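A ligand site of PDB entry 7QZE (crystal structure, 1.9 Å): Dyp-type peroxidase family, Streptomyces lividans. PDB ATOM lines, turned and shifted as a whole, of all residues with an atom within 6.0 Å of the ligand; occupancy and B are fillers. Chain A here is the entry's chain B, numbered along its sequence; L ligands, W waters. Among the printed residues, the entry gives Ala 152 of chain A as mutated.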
ATOM      1  N   ASP A 146      15.380 -24.641 -13.673  1.00  0.00           N
ATOM      2  CA  ASP A 146      16.790 -24.451 -13.291  1.00  0.00           C
ATOM      3  C   ASP A 146      17.688 -25.240 -14.255  1.00  0.00           C
ATOM      4  O   ASP A 146      17.183 -25.776 -15.262  1.00  0.00           O
ATOM      5  CB  ASP A 146      17.006 -24.828 -11.825  1.00  0.00           C
ATOM      6  CG  ASP A 146      16.793 -26.308 -11.504  1.00  0.00           C
ATOM      7  OD1 ASP A 146      16.726 -27.154 -12.466  1.00  0.00           O
ATOM      8  OD2 ASP A 146      16.643 -26.583 -10.281  1.00  0.00           O
ATOM      9  N   LEU A 148      19.078 -28.026 -13.953  1.00  0.00           N
ATOM     10  CA  LEU A 148      18.790 -29.495 -13.996  1.00  0.00           C
ATOM     11  C   LEU A 148      17.458 -29.795 -14.695  1.00  0.00           C
ATOM     12  O   LEU A 148      17.129 -30.967 -14.849  1.00  0.00           O
ATOM     13  CB  LEU A 148      18.767 -30.017 -12.556  1.00  0.00           C
ATOM     14  CG  LEU A 148      20.072 -29.850 -11.762  1.00  0.00           C
ATOM     15  CD1 LEU A 148      19.917 -30.545 -10.426  1.00  0.00           C
ATOM     16  CD2 LEU A 148      21.279 -30.390 -12.523  1.00  0.00           C
ATOM     17  N   PHE A 150      14.386 -28.690 -13.696  1.00  0.00           N
ATOM     18  CA  PHE A 150      13.251 -28.727 -12.742  1.00  0.00           C
ATOM     19  C   PHE A 150      12.757 -27.310 -12.427  1.00  0.00           C
ATOM     20  O   PHE A 150      13.564 -26.370 -12.369  1.00  0.00           O
ATOM     21  CB  PHE A 150      13.653 -29.442 -11.450  1.00  0.00           C
ATOM     22  CG  PHE A 150      13.607 -30.946 -11.585  1.00  0.00           C
ATOM     23  CD1 PHE A 150      14.553 -31.606 -12.346  1.00  0.00           C
ATOM     24  CD2 PHE A 150      12.606 -31.678 -10.976  1.00  0.00           C
ATOM     25  CE1 PHE A 150      14.483 -32.991 -12.511  1.00  0.00           C
ATOM     26  CE2 PHE A 150      12.541 -33.056 -11.144  1.00  0.00           C
ATOM     27  CZ  PHE A 150      13.484 -33.710 -11.898  1.00  0.00           C
ATOM     28  N   VAL A 151      11.456 -27.160 -12.196  1.00  0.00           N
ATOM     29  CA  VAL A 151      10.845 -25.875 -11.747  1.00  0.00           C
ATOM     30  C   VAL A 151      11.481 -25.534 -10.390  1.00  0.00           C
ATOM     31  O   VAL A 151      11.570 -26.410  -9.521  1.00  0.00           O
ATOM     32  CB  VAL A 151       9.315 -25.994 -11.698  1.00  0.00           C
ATOM     33  CG1 VAL A 151       8.644 -24.788 -11.076  1.00  0.00           C
ATOM     34  CG2 VAL A 151       8.752 -26.256 -13.080  1.00  0.00           C
ATOM     35  N   ALA A 152      11.887 -24.282 -10.194  1.00  0.00           N
ATOM     36  CA  ALA A 152      12.651 -23.843  -9.007  1.00  0.00           C
ATOM     37  C   ALA A 152      11.917 -22.709  -8.295  1.00  0.00           C
ATOM     38  O   ALA A 152      11.690 -21.707  -8.935  1.00  0.00           O
ATOM     39  CB  ALA A 152      14.018 -23.382  -9.408  1.00  0.00           C
ATOM     40  N   GLY A 153      11.664 -22.868  -6.991  1.00  0.00           N
ATOM     41  CA  GLY A 153      11.065 -21.834  -6.125  1.00  0.00           C
ATOM     42  C   GLY A 153       9.712 -22.255  -5.576  1.00  0.00           C
ATOM     43  O   GLY A 153       9.208 -21.591  -4.679  1.00  0.00           O
ATOM     44  N   THR A 154       9.181 -23.391  -6.025  1.00  0.00           N
ATOM     45  CA  THR A 154       7.771 -23.805  -5.793  1.00  0.00           C
ATOM     46  C   THR A 154       7.365 -23.652  -4.322  1.00  0.00           C
ATOM     47  O   THR A 154       6.274 -23.073  -4.072  1.00  0.00           O
ATOM     48  CB  THR A 154       7.542 -25.250  -6.256  1.00  0.00           C
ATOM     49  OG1 THR A 154       7.994 -25.336  -7.613  1.00  0.00           O
ATOM     50  CG2 THR A 154       6.101 -25.698  -6.182  1.00  0.00           C
ATOM     51  N   GLU A 155       8.182 -24.172  -3.393  1.00  0.00           N
ATOM     52  CA  GLU A 155       7.792 -24.310  -1.954  1.00  0.00           C
ATOM     53  C   GLU A 155       8.334 -23.140  -1.135  1.00  0.00           C
ATOM     54  O   GLU A 155       8.281 -23.231   0.102  1.00  0.00           O
ATOM     55  CB  GLU A 155       8.222 -25.682  -1.419  1.00  0.00           C
ATOM     56  CG  GLU A 155       7.281 -26.773  -1.895  1.00  0.00           C
ATOM     57  CD  GLU A 155       5.808 -26.554  -1.528  1.00  0.00           C
ATOM     58  OE1 GLU A 155       5.532 -26.300  -0.372  1.00  0.00           O
ATOM     59  OE2 GLU A 155       4.950 -26.564  -2.424  1.00  0.00           O
ATOM     60  N   ASN A 156       8.782 -22.064  -1.771  1.00  0.00           N
ATOM     61  CA  ASN A 156       9.176 -20.825  -1.052  1.00  0.00           C
ATOM     62  C   ASN A 156       7.961 -20.311  -0.275  1.00  0.00           C
ATOM     63  O   ASN A 156       6.851 -20.303  -0.799  1.00  0.00           O
ATOM     64  CB  ASN A 156       9.626 -19.720  -2.006  1.00  0.00           C
ATOM     65  CG  ASN A 156      11.117 -19.672  -2.256  1.00  0.00           C
ATOM     66  OD1 ASN A 156      11.918 -20.093  -1.417  1.00  0.00           O
ATOM     67  ND2 ASN A 156      11.492 -19.118  -3.398  1.00  0.00           N
ATOM     68  N   GLN A 184      26.122 -20.148  -2.006  1.00  0.00           N
ATOM     69  CA  GLN A 184      27.036 -21.213  -2.481  1.00  0.00           C
ATOM     70  C   GLN A 184      26.909 -21.250  -4.004  1.00  0.00           C
ATOM     71  O   GLN A 184      25.788 -21.348  -4.495  1.00  0.00           O
ATOM     72  CB  GLN A 184      26.697 -22.595  -1.945  1.00  0.00           C
ATOM     73  CG  GLN A 184      26.761 -22.743  -0.448  1.00  0.00           C
ATOM     74  CD  GLN A 184      26.312 -24.134  -0.108  1.00  0.00           C
ATOM     75  OE1 GLN A 184      25.141 -24.479  -0.238  1.00  0.00           O
ATOM     76  NE2 GLN A 184      27.239 -24.961   0.332  1.00  0.00           N
ATOM     77  N   TYR A 186      27.317 -23.513  -7.084  1.00  0.00           N
ATOM     78  CA  TYR A 186      27.453 -24.951  -7.408  1.00  0.00           C
ATOM     79  C   TYR A 186      27.764 -25.096  -8.887  1.00  0.00           C
ATOM     80  O   TYR A 186      27.119 -24.388  -9.706  1.00  0.00           O
ATOM     81  CB  TYR A 186      26.163 -25.703  -7.091  1.00  0.00           C
ATOM     82  CG  TYR A 186      25.909 -25.963  -5.638  1.00  0.00           C
ATOM     83  CD1 TYR A 186      25.230 -25.050  -4.850  1.00  0.00           C
ATOM     84  CD2 TYR A 186      26.368 -27.130  -5.054  1.00  0.00           C
ATOM     85  CE1 TYR A 186      24.998 -25.298  -3.513  1.00  0.00           C
ATOM     86  CE2 TYR A 186      26.121 -27.396  -3.723  1.00  0.00           C
ATOM     87  CZ  TYR A 186      25.443 -26.478  -2.952  1.00  0.00           C
ATOM     88  OH  TYR A 186      25.234 -26.794  -1.648  1.00  0.00           O
ATOM     89  N   HIS A 188      27.572 -28.149 -11.858  1.00  0.00           N
ATOM     90  CA  HIS A 188      26.906 -29.432 -12.118  1.00  0.00           C
ATOM     91  C   HIS A 188      27.751 -30.271 -13.069  1.00  0.00           C
ATOM     92  O   HIS A 188      28.378 -29.727 -13.991  1.00  0.00           O
ATOM     93  CB  HIS A 188      25.497 -29.203 -12.680  1.00  0.00           C
ATOM     94  CG  HIS A 188      24.598 -28.507 -11.728  1.00  0.00           C
ATOM     95  ND1 HIS A 188      24.257 -29.080 -10.519  1.00  0.00           N
ATOM     96  CD2 HIS A 188      23.981 -27.308 -11.792  1.00  0.00           C
ATOM     97  CE1 HIS A 188      23.486 -28.234  -9.853  1.00  0.00           C
ATOM     98  NE2 HIS A 188      23.291 -27.148 -10.604  1.00  0.00           N
ATOM     99  N   ILE A 205      15.390 -35.382  -6.887  1.00  0.00           N
ATOM    100  CA  ILE A 205      14.780 -34.062  -6.475  1.00  0.00           C
ATOM    101  C   ILE A 205      13.665 -34.304  -5.458  1.00  0.00           C
ATOM    102  O   ILE A 205      13.665 -33.637  -4.424  1.00  0.00           O
ATOM    103  CB  ILE A 205      14.295 -33.262  -7.694  1.00  0.00           C
ATOM    104  CG1 ILE A 205      15.438 -32.965  -8.686  1.00  0.00           C
ATOM    105  CG2 ILE A 205      13.574 -32.000  -7.263  1.00  0.00           C
ATOM    106  CD1 ILE A 205      16.567 -32.127  -8.120  1.00  0.00           C
ATOM    107  N   ARG A 207      10.309 -34.376  -6.697  1.00  0.00           N
ATOM    108  CA  ARG A 207       9.116 -33.819  -7.411  1.00  0.00           C
ATOM    109  C   ARG A 207       9.112 -34.384  -8.844  1.00  0.00           C
ATOM    110  O   ARG A 207      10.216 -34.784  -9.346  1.00  0.00           O
ATOM    111  CB  ARG A 207       9.115 -32.287  -7.433  1.00  0.00           C
ATOM    112  CG  ARG A 207       9.421 -31.629  -6.091  1.00  0.00           C
ATOM    113  CD  ARG A 207       9.282 -30.087  -6.128  1.00  0.00           C
ATOM    114  NE  ARG A 207       7.873 -29.721  -6.306  1.00  0.00           N
ATOM    115  CZ  ARG A 207       6.976 -29.480  -5.343  1.00  0.00           C
ATOM    116  NH1 ARG A 207       5.727 -29.207  -5.672  1.00  0.00           N
ATOM    117  NH2 ARG A 207       7.314 -29.426  -4.079  1.00  0.00           N
ATOM    118  N   ASP A 212       5.761 -30.819 -11.805  1.00  0.00           N
ATOM    119  CA  ASP A 212       6.251 -30.162 -10.565  1.00  0.00           C
ATOM    120  C   ASP A 212       5.392 -30.612  -9.368  1.00  0.00           C
ATOM    121  O   ASP A 212       5.430 -29.938  -8.348  1.00  0.00           O
ATOM    122  CB  ASP A 212       6.302 -28.640 -10.740  1.00  0.00           C
ATOM    123  CG  ASP A 212       6.834 -27.838  -9.573  1.00  0.00           C
ATOM    124  OD1 ASP A 212       7.853 -28.258  -8.992  1.00  0.00           O
ATOM    125  OD2 ASP A 212       6.197 -26.787  -9.267  1.00  0.00           O
ATOM    126  N   GLU A 214       4.754 -32.808  -6.108  1.00  0.00           N
ATOM    127  CA  GLU A 214       5.615 -33.474  -5.121  1.00  0.00           C
ATOM    128  C   GLU A 214       5.370 -34.990  -5.177  1.00  0.00           C
ATOM    129  O   GLU A 214       4.216 -35.416  -5.411  1.00  0.00           O
ATOM    130  CB  GLU A 214       5.306 -32.904  -3.748  1.00  0.00           C
ATOM    131  CG  GLU A 214       6.273 -33.380  -2.720  1.00  0.00           C
ATOM    132  CD  GLU A 214       6.260 -32.555  -1.453  1.00  0.00           C
ATOM    133  OE1 GLU A 214       5.947 -31.369  -1.521  1.00  0.00           O
ATOM    134  OE2 GLU A 214       6.580 -33.121  -0.420  1.00  0.00           O
ATOM    135  N   HIS A 225      16.400 -34.501  -2.372  1.00  0.00           N
ATOM    136  CA  HIS A 225      16.604 -33.077  -1.995  1.00  0.00           C
ATOM    137  C   HIS A 225      15.440 -32.565  -1.145  1.00  0.00           C
ATOM    138  O   HIS A 225      15.675 -31.957  -0.058  1.00  0.00           O
ATOM    139  CB  HIS A 225      16.801 -32.240  -3.259  1.00  0.00           C
ATOM    140  CG  HIS A 225      17.222 -30.857  -2.941  1.00  0.00           C
ATOM    141  ND1 HIS A 225      18.302 -30.594  -2.156  1.00  0.00           N
ATOM    142  CD2 HIS A 225      16.747 -29.668  -3.379  1.00  0.00           C
ATOM    143  CE1 HIS A 225      18.477 -29.282  -2.090  1.00  0.00           C
ATOM    144  NE2 HIS A 225      17.517 -28.703  -2.836  1.00  0.00           N
ATOM    145  N   VAL A 226      14.216 -32.834  -1.598  1.00  0.00           N
ATOM    146  CA  VAL A 226      13.001 -32.321  -0.913  1.00  0.00           C
ATOM    147  C   VAL A 226      12.914 -32.974   0.475  1.00  0.00           C
ATOM    148  O   VAL A 226      12.579 -32.257   1.433  1.00  0.00           O
ATOM    149  CB  VAL A 226      11.741 -32.513  -1.787  1.00  0.00           C
ATOM    150  CG1 VAL A 226      10.470 -32.399  -0.959  1.00  0.00           C
ATOM    151  CG2 VAL A 226      11.742 -31.520  -2.960  1.00  0.00           C
ATOM    152  N   THR A 229      15.766 -31.433   2.950  1.00  0.00           N
ATOM    153  CA  THR A 229      15.670 -29.972   3.210  1.00  0.00           C
ATOM    154  C   THR A 229      14.310 -29.639   3.843  1.00  0.00           C
ATOM    155  O   THR A 229      14.012 -28.437   4.018  1.00  0.00           O
ATOM    156  CB  THR A 229      15.976 -29.149   1.965  1.00  0.00           C
ATOM    157  OG1 THR A 229      15.089 -29.501   0.909  1.00  0.00           O
ATOM    158  CG2 THR A 229      17.403 -29.343   1.494  1.00  0.00           C
ATOM    159  N   SER A 230      13.512 -30.645   4.123  1.00  0.00           N
ATOM    160  CA  SER A 230      12.252 -30.542   4.911  1.00  0.00           C
ATOM    161  C   SER A 230      12.619 -30.729   6.372  1.00  0.00           C
ATOM    162  O   SER A 230      13.060 -31.840   6.700  1.00  0.00           O
ATOM    163  CB  SER A 230      11.262 -31.602   4.522  1.00  0.00           C
ATOM    164  OG  SER A 230      10.860 -31.400   3.192  1.00  0.00           O
ATOM    165  N   ILE A 241      13.029 -21.412   4.651  1.00  0.00           N
ATOM    166  CA  ILE A 241      13.922 -20.337   4.143  1.00  0.00           C
ATOM    167  C   ILE A 241      13.325 -19.829   2.837  1.00  0.00           C
ATOM    168  O   ILE A 241      12.424 -20.464   2.327  1.00  0.00           O
ATOM    169  CB  ILE A 241      15.365 -20.854   3.988  1.00  0.00           C
ATOM    170  CG1 ILE A 241      15.518 -21.924   2.903  1.00  0.00           C
ATOM    171  CG2 ILE A 241      15.861 -21.377   5.340  1.00  0.00           C
ATOM    172  CD1 ILE A 241      16.963 -22.185   2.515  1.00  0.00           C
ATOM    173  N   ARG A 243      14.486 -18.924  -1.024  1.00  0.00           N
ATOM    174  CA  ARG A 243      15.607 -19.194  -1.975  1.00  0.00           C
ATOM    175  C   ARG A 243      15.370 -18.476  -3.301  1.00  0.00           C
ATOM    176  O   ARG A 243      14.225 -18.477  -3.780  1.00  0.00           O
ATOM    177  CB  ARG A 243      15.692 -20.699  -2.208  1.00  0.00           C
ATOM    178  CG  ARG A 243      15.871 -21.503  -0.936  1.00  0.00           C
ATOM    179  CD  ARG A 243      15.545 -22.977  -1.109  1.00  0.00           C
ATOM    180  NE  ARG A 243      14.119 -23.142  -1.216  1.00  0.00           N
ATOM    181  CZ  ARG A 243      13.454 -23.550  -2.291  1.00  0.00           C
ATOM    182  NH1 ARG A 243      14.110 -23.896  -3.401  1.00  0.00           N
ATOM    183  NH2 ARG A 243      12.128 -23.595  -2.258  1.00  0.00           N
ATOM    184  N   ASN A 245      17.545 -19.011  -6.169  1.00  0.00           N
ATOM    185  CA  ASN A 245      18.585 -19.741  -6.919  1.00  0.00           C
ATOM    186  C   ASN A 245      18.527 -19.326  -8.409  1.00  0.00           C
ATOM    187  O   ASN A 245      17.429 -19.197  -8.960  1.00  0.00           O
ATOM    188  CB  ASN A 245      18.445 -21.271  -6.842  1.00  0.00           C
ATOM    189  CG  ASN A 245      18.447 -21.847  -5.431  1.00  0.00           C
ATOM    190  OD1 ASN A 245      18.587 -21.126  -4.440  1.00  0.00           O
ATOM    191  ND2 ASN A 245      18.311 -23.153  -5.330  1.00  0.00           N
ATOM    192  N   THR A 258      24.372 -23.643 -10.703  1.00  0.00           N
ATOM    193  CA  THR A 258      23.284 -23.051  -9.902  1.00  0.00           C
ATOM    194  C   THR A 258      23.937 -22.151  -8.856  1.00  0.00           C
ATOM    195  O   THR A 258      24.817 -22.647  -8.099  1.00  0.00           O
ATOM    196  CB  THR A 258      22.445 -24.130  -9.199  1.00  0.00           C
ATOM    197  OG1 THR A 258      21.782 -24.906 -10.181  1.00  0.00           O
ATOM    198  CG2 THR A 258      21.389 -23.549  -8.285  1.00  0.00           C
ATOM    199  N   PHE A 260      23.218 -20.718  -5.517  1.00  0.00           N
ATOM    200  CA  PHE A 260      22.253 -20.868  -4.409  1.00  0.00           C
ATOM    201  C   PHE A 260      22.312 -19.612  -3.547  1.00  0.00           C
ATOM    202  O   PHE A 260      23.445 -19.194  -3.213  1.00  0.00           O
ATOM    203  CB  PHE A 260      22.542 -22.104  -3.563  1.00  0.00           C
ATOM    204  CG  PHE A 260      21.769 -22.096  -2.264  1.00  0.00           C
ATOM    205  CD1 PHE A 260      20.457 -22.562  -2.238  1.00  0.00           C
ATOM    206  CD2 PHE A 260      22.332 -21.621  -1.097  1.00  0.00           C
ATOM    207  CE1 PHE A 260      19.742 -22.554  -1.057  1.00  0.00           C
ATOM    208  CE2 PHE A 260      21.586 -21.569   0.078  1.00  0.00           C
ATOM    209  CZ  PHE A 260      20.305 -22.049   0.088  1.00  0.00           C
ATOM    210  N   THR A 270      19.184 -22.584   7.901  1.00  0.00           N
ATOM    211  CA  THR A 270      19.939 -22.895   6.666  1.00  0.00           C
ATOM    212  C   THR A 270      21.064 -23.891   6.987  1.00  0.00           C
ATOM    213  O   THR A 270      21.253 -24.861   6.197  1.00  0.00           O
ATOM    214  CB  THR A 270      20.451 -21.600   6.019  1.00  0.00           C
ATOM    215  OG1 THR A 270      19.411 -20.622   6.060  1.00  0.00           O
ATOM    216  CG2 THR A 270      20.928 -21.828   4.605  1.00  0.00           C
ATOM    217  N   MET A 273      19.797 -27.439   7.387  1.00  0.00           N
ATOM    218  CA  MET A 273      19.488 -28.034   6.065  1.00  0.00           C
ATOM    219  C   MET A 273      20.792 -28.505   5.440  1.00  0.00           C
ATOM    220  O   MET A 273      20.784 -29.615   4.912  1.00  0.00           O
ATOM    221  CB  MET A 273      18.766 -27.054   5.137  1.00  0.00           C
ATOM    222  CG  MET A 273      17.362 -26.768   5.589  1.00  0.00           C
ATOM    223  SD  MET A 273      16.595 -25.436   4.638  1.00  0.00           S
ATOM    224  CE  MET A 273      14.968 -25.501   5.387  1.00  0.00           C
ATOM    225  N   LEU A 274      21.835 -27.667   5.450  1.00  0.00           N
ATOM    226  CA  LEU A 274      23.171 -27.972   4.904  1.00  0.00           C
ATOM    227  C   LEU A 274      23.774 -29.200   5.632  1.00  0.00           C
ATOM    228  O   LEU A 274      24.342 -30.024   4.941  1.00  0.00           O
ATOM    229  CB  LEU A 274      24.080 -26.748   4.985  1.00  0.00           C
ATOM    230  CG  LEU A 274      23.797 -25.638   3.971  1.00  0.00           C
ATOM    231  CD1 LEU A 274      24.606 -24.396   4.296  1.00  0.00           C
ATOM    232  CD2 LEU A 274      24.104 -26.077   2.543  1.00  0.00           C
ATOM    233  N   MET A 277      22.072 -32.277   4.289  1.00  0.00           N
ATOM    234  CA  MET A 277      22.533 -32.449   2.894  1.00  0.00           C
ATOM    235  C   MET A 277      23.924 -33.071   2.830  1.00  0.00           C
ATOM    236  O   MET A 277      24.111 -34.081   2.093  1.00  0.00           O
ATOM    237  CB  MET A 277      22.518 -31.085   2.179  1.00  0.00           C
ATOM    238  CG  MET A 277      21.110 -30.593   1.848  1.00  0.00           C
ATOM    239  SD  MET A 277      21.185 -29.032   0.927  1.00  0.00           S
ATOM    240  CE  MET A 277      21.969 -29.567  -0.578  1.00  0.00           C
ATOM    241  N   PHE A 278      24.902 -32.506   3.539  1.00  0.00           N
ATOM    242  CA  PHE A 278      26.318 -32.897   3.399  1.00  0.00           C
ATOM    243  C   PHE A 278      26.706 -34.053   4.348  1.00  0.00           C
ATOM    244  O   PHE A 278      27.591 -34.801   3.974  1.00  0.00           O
ATOM    245  CB  PHE A 278      27.198 -31.679   3.629  1.00  0.00           C
ATOM    246  CG  PHE A 278      27.239 -30.783   2.438  1.00  0.00           C
ATOM    247  CD1 PHE A 278      28.206 -30.967   1.478  1.00  0.00           C
ATOM    248  CD2 PHE A 278      26.278 -29.792   2.244  1.00  0.00           C
ATOM    249  CE1 PHE A 278      28.232 -30.178   0.343  1.00  0.00           C
ATOM    250  CE2 PHE A 278      26.322 -28.989   1.108  1.00  0.00           C
ATOM    251  CZ  PHE A 278      27.310 -29.177   0.172  1.00  0.00           C
ATOM    252  N   ILE A 289      21.322 -34.796  -4.683  1.00  0.00           N
ATOM    253  CA  ILE A 289      21.640 -33.663  -5.598  1.00  0.00           C
ATOM    254  C   ILE A 289      23.159 -33.396  -5.588  1.00  0.00           C
ATOM    255  O   ILE A 289      23.699 -32.936  -6.631  1.00  0.00           O
ATOM    256  CB  ILE A 289      20.771 -32.421  -5.294  1.00  0.00           C
ATOM    257  CG1 ILE A 289      20.452 -31.644  -6.581  1.00  0.00           C
ATOM    258  CG2 ILE A 289      21.432 -31.548  -4.238  1.00  0.00           C
ATOM    259  CD1 ILE A 289      19.461 -30.531  -6.355  1.00  0.00           C
ATOM    260  N   SER A 293      26.379 -32.110  -8.195  1.00  0.00           N
ATOM    261  CA  SER A 293      26.577 -30.672  -7.857  1.00  0.00           C
ATOM    262  C   SER A 293      27.721 -30.545  -6.869  1.00  0.00           C
ATOM    263  O   SER A 293      27.588 -31.130  -5.783  1.00  0.00           O
ATOM    264  CB  SER A 293      25.331 -30.120  -7.251  1.00  0.00           C
ATOM    265  OG  SER A 293      24.191 -30.541  -7.963  1.00  0.00           O
HETATM  266  C1  LIG L   1      13.682 -27.277  -3.095  1.00  0.00           C
HETATM  267  C2  LIG L   1      16.992 -27.216  -6.652  1.00  0.00           C
HETATM  268  C3  LIG L   1      20.405 -26.308  -3.345  1.00  0.00           C
HETATM  269  C4  LIG L   1      17.060 -25.862   0.058  1.00  0.00           C
HETATM  270  C5  LIG L   1      14.296 -27.395  -4.334  1.00  0.00           C
HETATM  271  C6  LIG L   1      13.616 -27.761  -5.549  1.00  0.00           C
HETATM  272  C7  LIG L   1      14.534 -27.744  -6.531  1.00  0.00           C
HETATM  273  C8  LIG L   1      15.778 -27.337  -5.959  1.00  0.00           C
HETATM  274  C9  LIG L   1      14.317 -28.070  -8.005  1.00  0.00           C
HETATM  275  C10 LIG L   1      12.140 -28.131  -5.675  1.00  0.00           C
HETATM  276  C11 LIG L   1      11.222 -26.925  -6.017  1.00  0.00           C
HETATM  277  C12 LIG L   1      11.402 -25.807  -5.018  1.00  0.00           C
HETATM  278  O1  LIG L   1      12.247 -24.875  -5.276  1.00  0.00           O
HETATM  279  O2  LIG L   1      10.698 -25.853  -3.975  1.00  0.00           O
HETATM  280  C13 LIG L   1      18.228 -26.954  -6.073  1.00  0.00           C
HETATM  281  C14 LIG L   1      19.498 -26.966  -6.752  1.00  0.00           C
HETATM  282  C15 LIG L   1      20.445 -26.710  -5.798  1.00  0.00           C
HETATM  283  C16 LIG L   1      19.747 -26.608  -4.520  1.00  0.00           C
HETATM  284  C17 LIG L   1      19.765 -27.163  -8.213  1.00  0.00           C
HETATM  285  C18 LIG L   1      21.909 -26.655  -5.804  1.00  0.00           C
HETATM  286  C19 LIG L   1      22.563 -27.279  -6.730  1.00  0.00           C
HETATM  287  C20 LIG L   1      19.822 -26.095  -2.135  1.00  0.00           C
HETATM  288  C21 LIG L   1      20.485 -25.875  -0.901  1.00  0.00           C
HETATM  289  C22 LIG L   1      19.516 -25.789   0.064  1.00  0.00           C
HETATM  290  C23 LIG L   1      18.271 -25.913  -0.593  1.00  0.00           C
HETATM  291  C24 LIG L   1      21.978 -25.738  -0.758  1.00  0.00           C
HETATM  292  C25 LIG L   1      19.608 -25.472   1.529  1.00  0.00           C
HETATM  293  C26 LIG L   1      20.707 -25.160   2.132  1.00  0.00           C
HETATM  294  C27 LIG L   1      15.877 -26.220  -0.574  1.00  0.00           C
HETATM  295  C28 LIG L   1      14.622 -26.222   0.186  1.00  0.00           C
HETATM  296  C29 LIG L   1      13.702 -26.629  -0.688  1.00  0.00           C
HETATM  297  C30 LIG L   1      14.395 -26.855  -1.970  1.00  0.00           C
HETATM  298  C31 LIG L   1      14.404 -25.882   1.671  1.00  0.00           C
HETATM  299  C32 LIG L   1      12.214 -26.810  -0.420  1.00  0.00           C
HETATM  300  C33 LIG L   1      11.882 -28.200   0.138  1.00  0.00           C
HETATM  301  C34 LIG L   1      10.399 -28.313   0.398  1.00  0.00           C
HETATM  302  O3  LIG L   1       9.599 -28.750  -0.481  1.00  0.00           O
HETATM  303  O4  LIG L   1      10.014 -27.976   1.553  1.00  0.00           O
HETATM  304  N1  LIG L   1      15.619 -27.133  -4.613  1.00  0.00           N
HETATM  305  N2  LIG L   1      18.448 -26.780  -4.775  1.00  0.00           N
HETATM  306  N3  LIG L   1      18.482 -26.159  -1.926  1.00  0.00           N
HETATM  307  N4  LIG L   1      15.713 -26.607  -1.865  1.00  0.00           N
HETATM  308 FE1  LIG L   1      17.029 -26.650  -3.269  1.00  0.00          FE
HETATM  309  O   HOH W   1       9.906 -28.426  -3.114  1.00  0.00           O
HETATM  310  O   HOH W   2      15.210 -24.107  -6.235  1.00  0.00           O
HETATM  311  O   HOH W   3      11.707 -26.860   3.544  1.00  0.00           O
HETATM  312  O   HOH W   4       7.378 -29.515   0.509  1.00  0.00           O
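The side-chain carboxylate (OD1) of Asp 212 is in salt-bridge range of the guanidinium group (NE) of Arg 207 (3.1 Å).
A ring nitrogen (NE2) of His 188 lies within hydrogen-bond range of the side-chain hydroxyl (OG1) of Thr 258 (2.7 Å).
O of Arg 243 sits at hydrogen-bond distance from ND2 of Asn 156, 2.8 Å away.
The side-chain hydroxyl of Ser 293 is in hydrogen-bond range of a ring nitrogen (ND1) of His 188 (2.9 Å).
The guanidinium group (NH2) of Arg 207 is in salt-bridge range of the side-chain carboxylate (OE1) of Glu 214, at 3.5 Å.
The backbone carbonyl oxygen (O) of His 225 is in hydrogen-bond range of the side-chain hydroxyl (OG1) of Thr 229 (2.7 Å).
O of Gln 184 lies within hydrogen-bond range of N of Phe 260, 2.8 Å away.
The backbone carbonyl oxygen (O) of Ile 289 is in hydrogen-bond range of the side-chain hydroxyl (OG) of Ser 293, at 2.8 Å.
Water W4 bridges an oxygen (O3) of the ligand and the side-chain carboxylate of Glu 214.
Water W1 lies within hydrogen-bond range of O3 of the ligand (2.7 Å) and NH2 of Arg 207 (2.9 Å).
Water W3 bridges the backbone carbonyl oxygen (O) of Thr 229 (2.8 Å) and an oxygen (O4) of the ligand (2.8 Å).
Water W2 lies within hydrogen-bond range of the guanidinium group of Arg 243 (3.0 Å), an oxygen (O1) of the ligand (3.2 Å) and the side-chain amide nitrogen of Asn 245 (3.4 Å).
OD2 of Asp 146 touches C9 of the ligand, 3.6 Å away.
Phe 150 touches the ligand.
Val 151 touches the ligand (O to C9, 3.5 Å).
Ala 152 touches the ligand.
OE1 of Gln 184 touches C24 of the ligand (3.4 Å).
Tyr 186 touches the ligand.
CE1 of His 188 touches C19 of the ligand, at 3.4 Å.
CD of Arg 207 touches C10 of the ligand, at 3.5 Å.
CG1 of Val 226 touches O3 of the ligand, 3.8 Å away.
Thr 229 touches the ligand.
OG of Ser 230 touches O4 of the ligand (3.9 Å).
ND2 of Asn 245 touches N2 of the ligand (3.7 Å).
OG1 of Thr 258 touches C17 of the ligand, at 3.6 Å.
Phe 260 touches the ligand.
Met 273 touches the ligand (SD to C31, 3.7 Å).
CD2 of Leu 274 touches C26 of the ligand, at 3.5 Å.
Met 277 touches the ligand (SD to C21, 3.7 Å).
Ile 289 touches the ligand (CD1 to C14, 3.6 Å).
OG of Ser 293 touches C19 of the ligand (3.8 Å).
Hydrophobic or aromatic side chains that line the ligand: Phe 150, Tyr 186, His 188, His 225, Val 226, Phe 260, Met 273, Leu 274, Met 277 and Ile 289.
The nearest printed residue that does not touch the ligand is Leu 148 (4.04 Å).
O1 of the ligand sits close to N of Thr 154 (3.5 Å).
NH1 of Arg 243 is in salt-bridge range of O1 of the ligand.
An iron atom (FE1) of the ligand is bound by a ring nitrogen (NE2) of His 225, at 2.2 Å.
O1 of the ligand lies within hydrogen-bond range of N of Gly 153, at 2.7 Å.
O2 of the ligand is in hydrogen-bond range of N of Glu 155 (3.1 Å).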
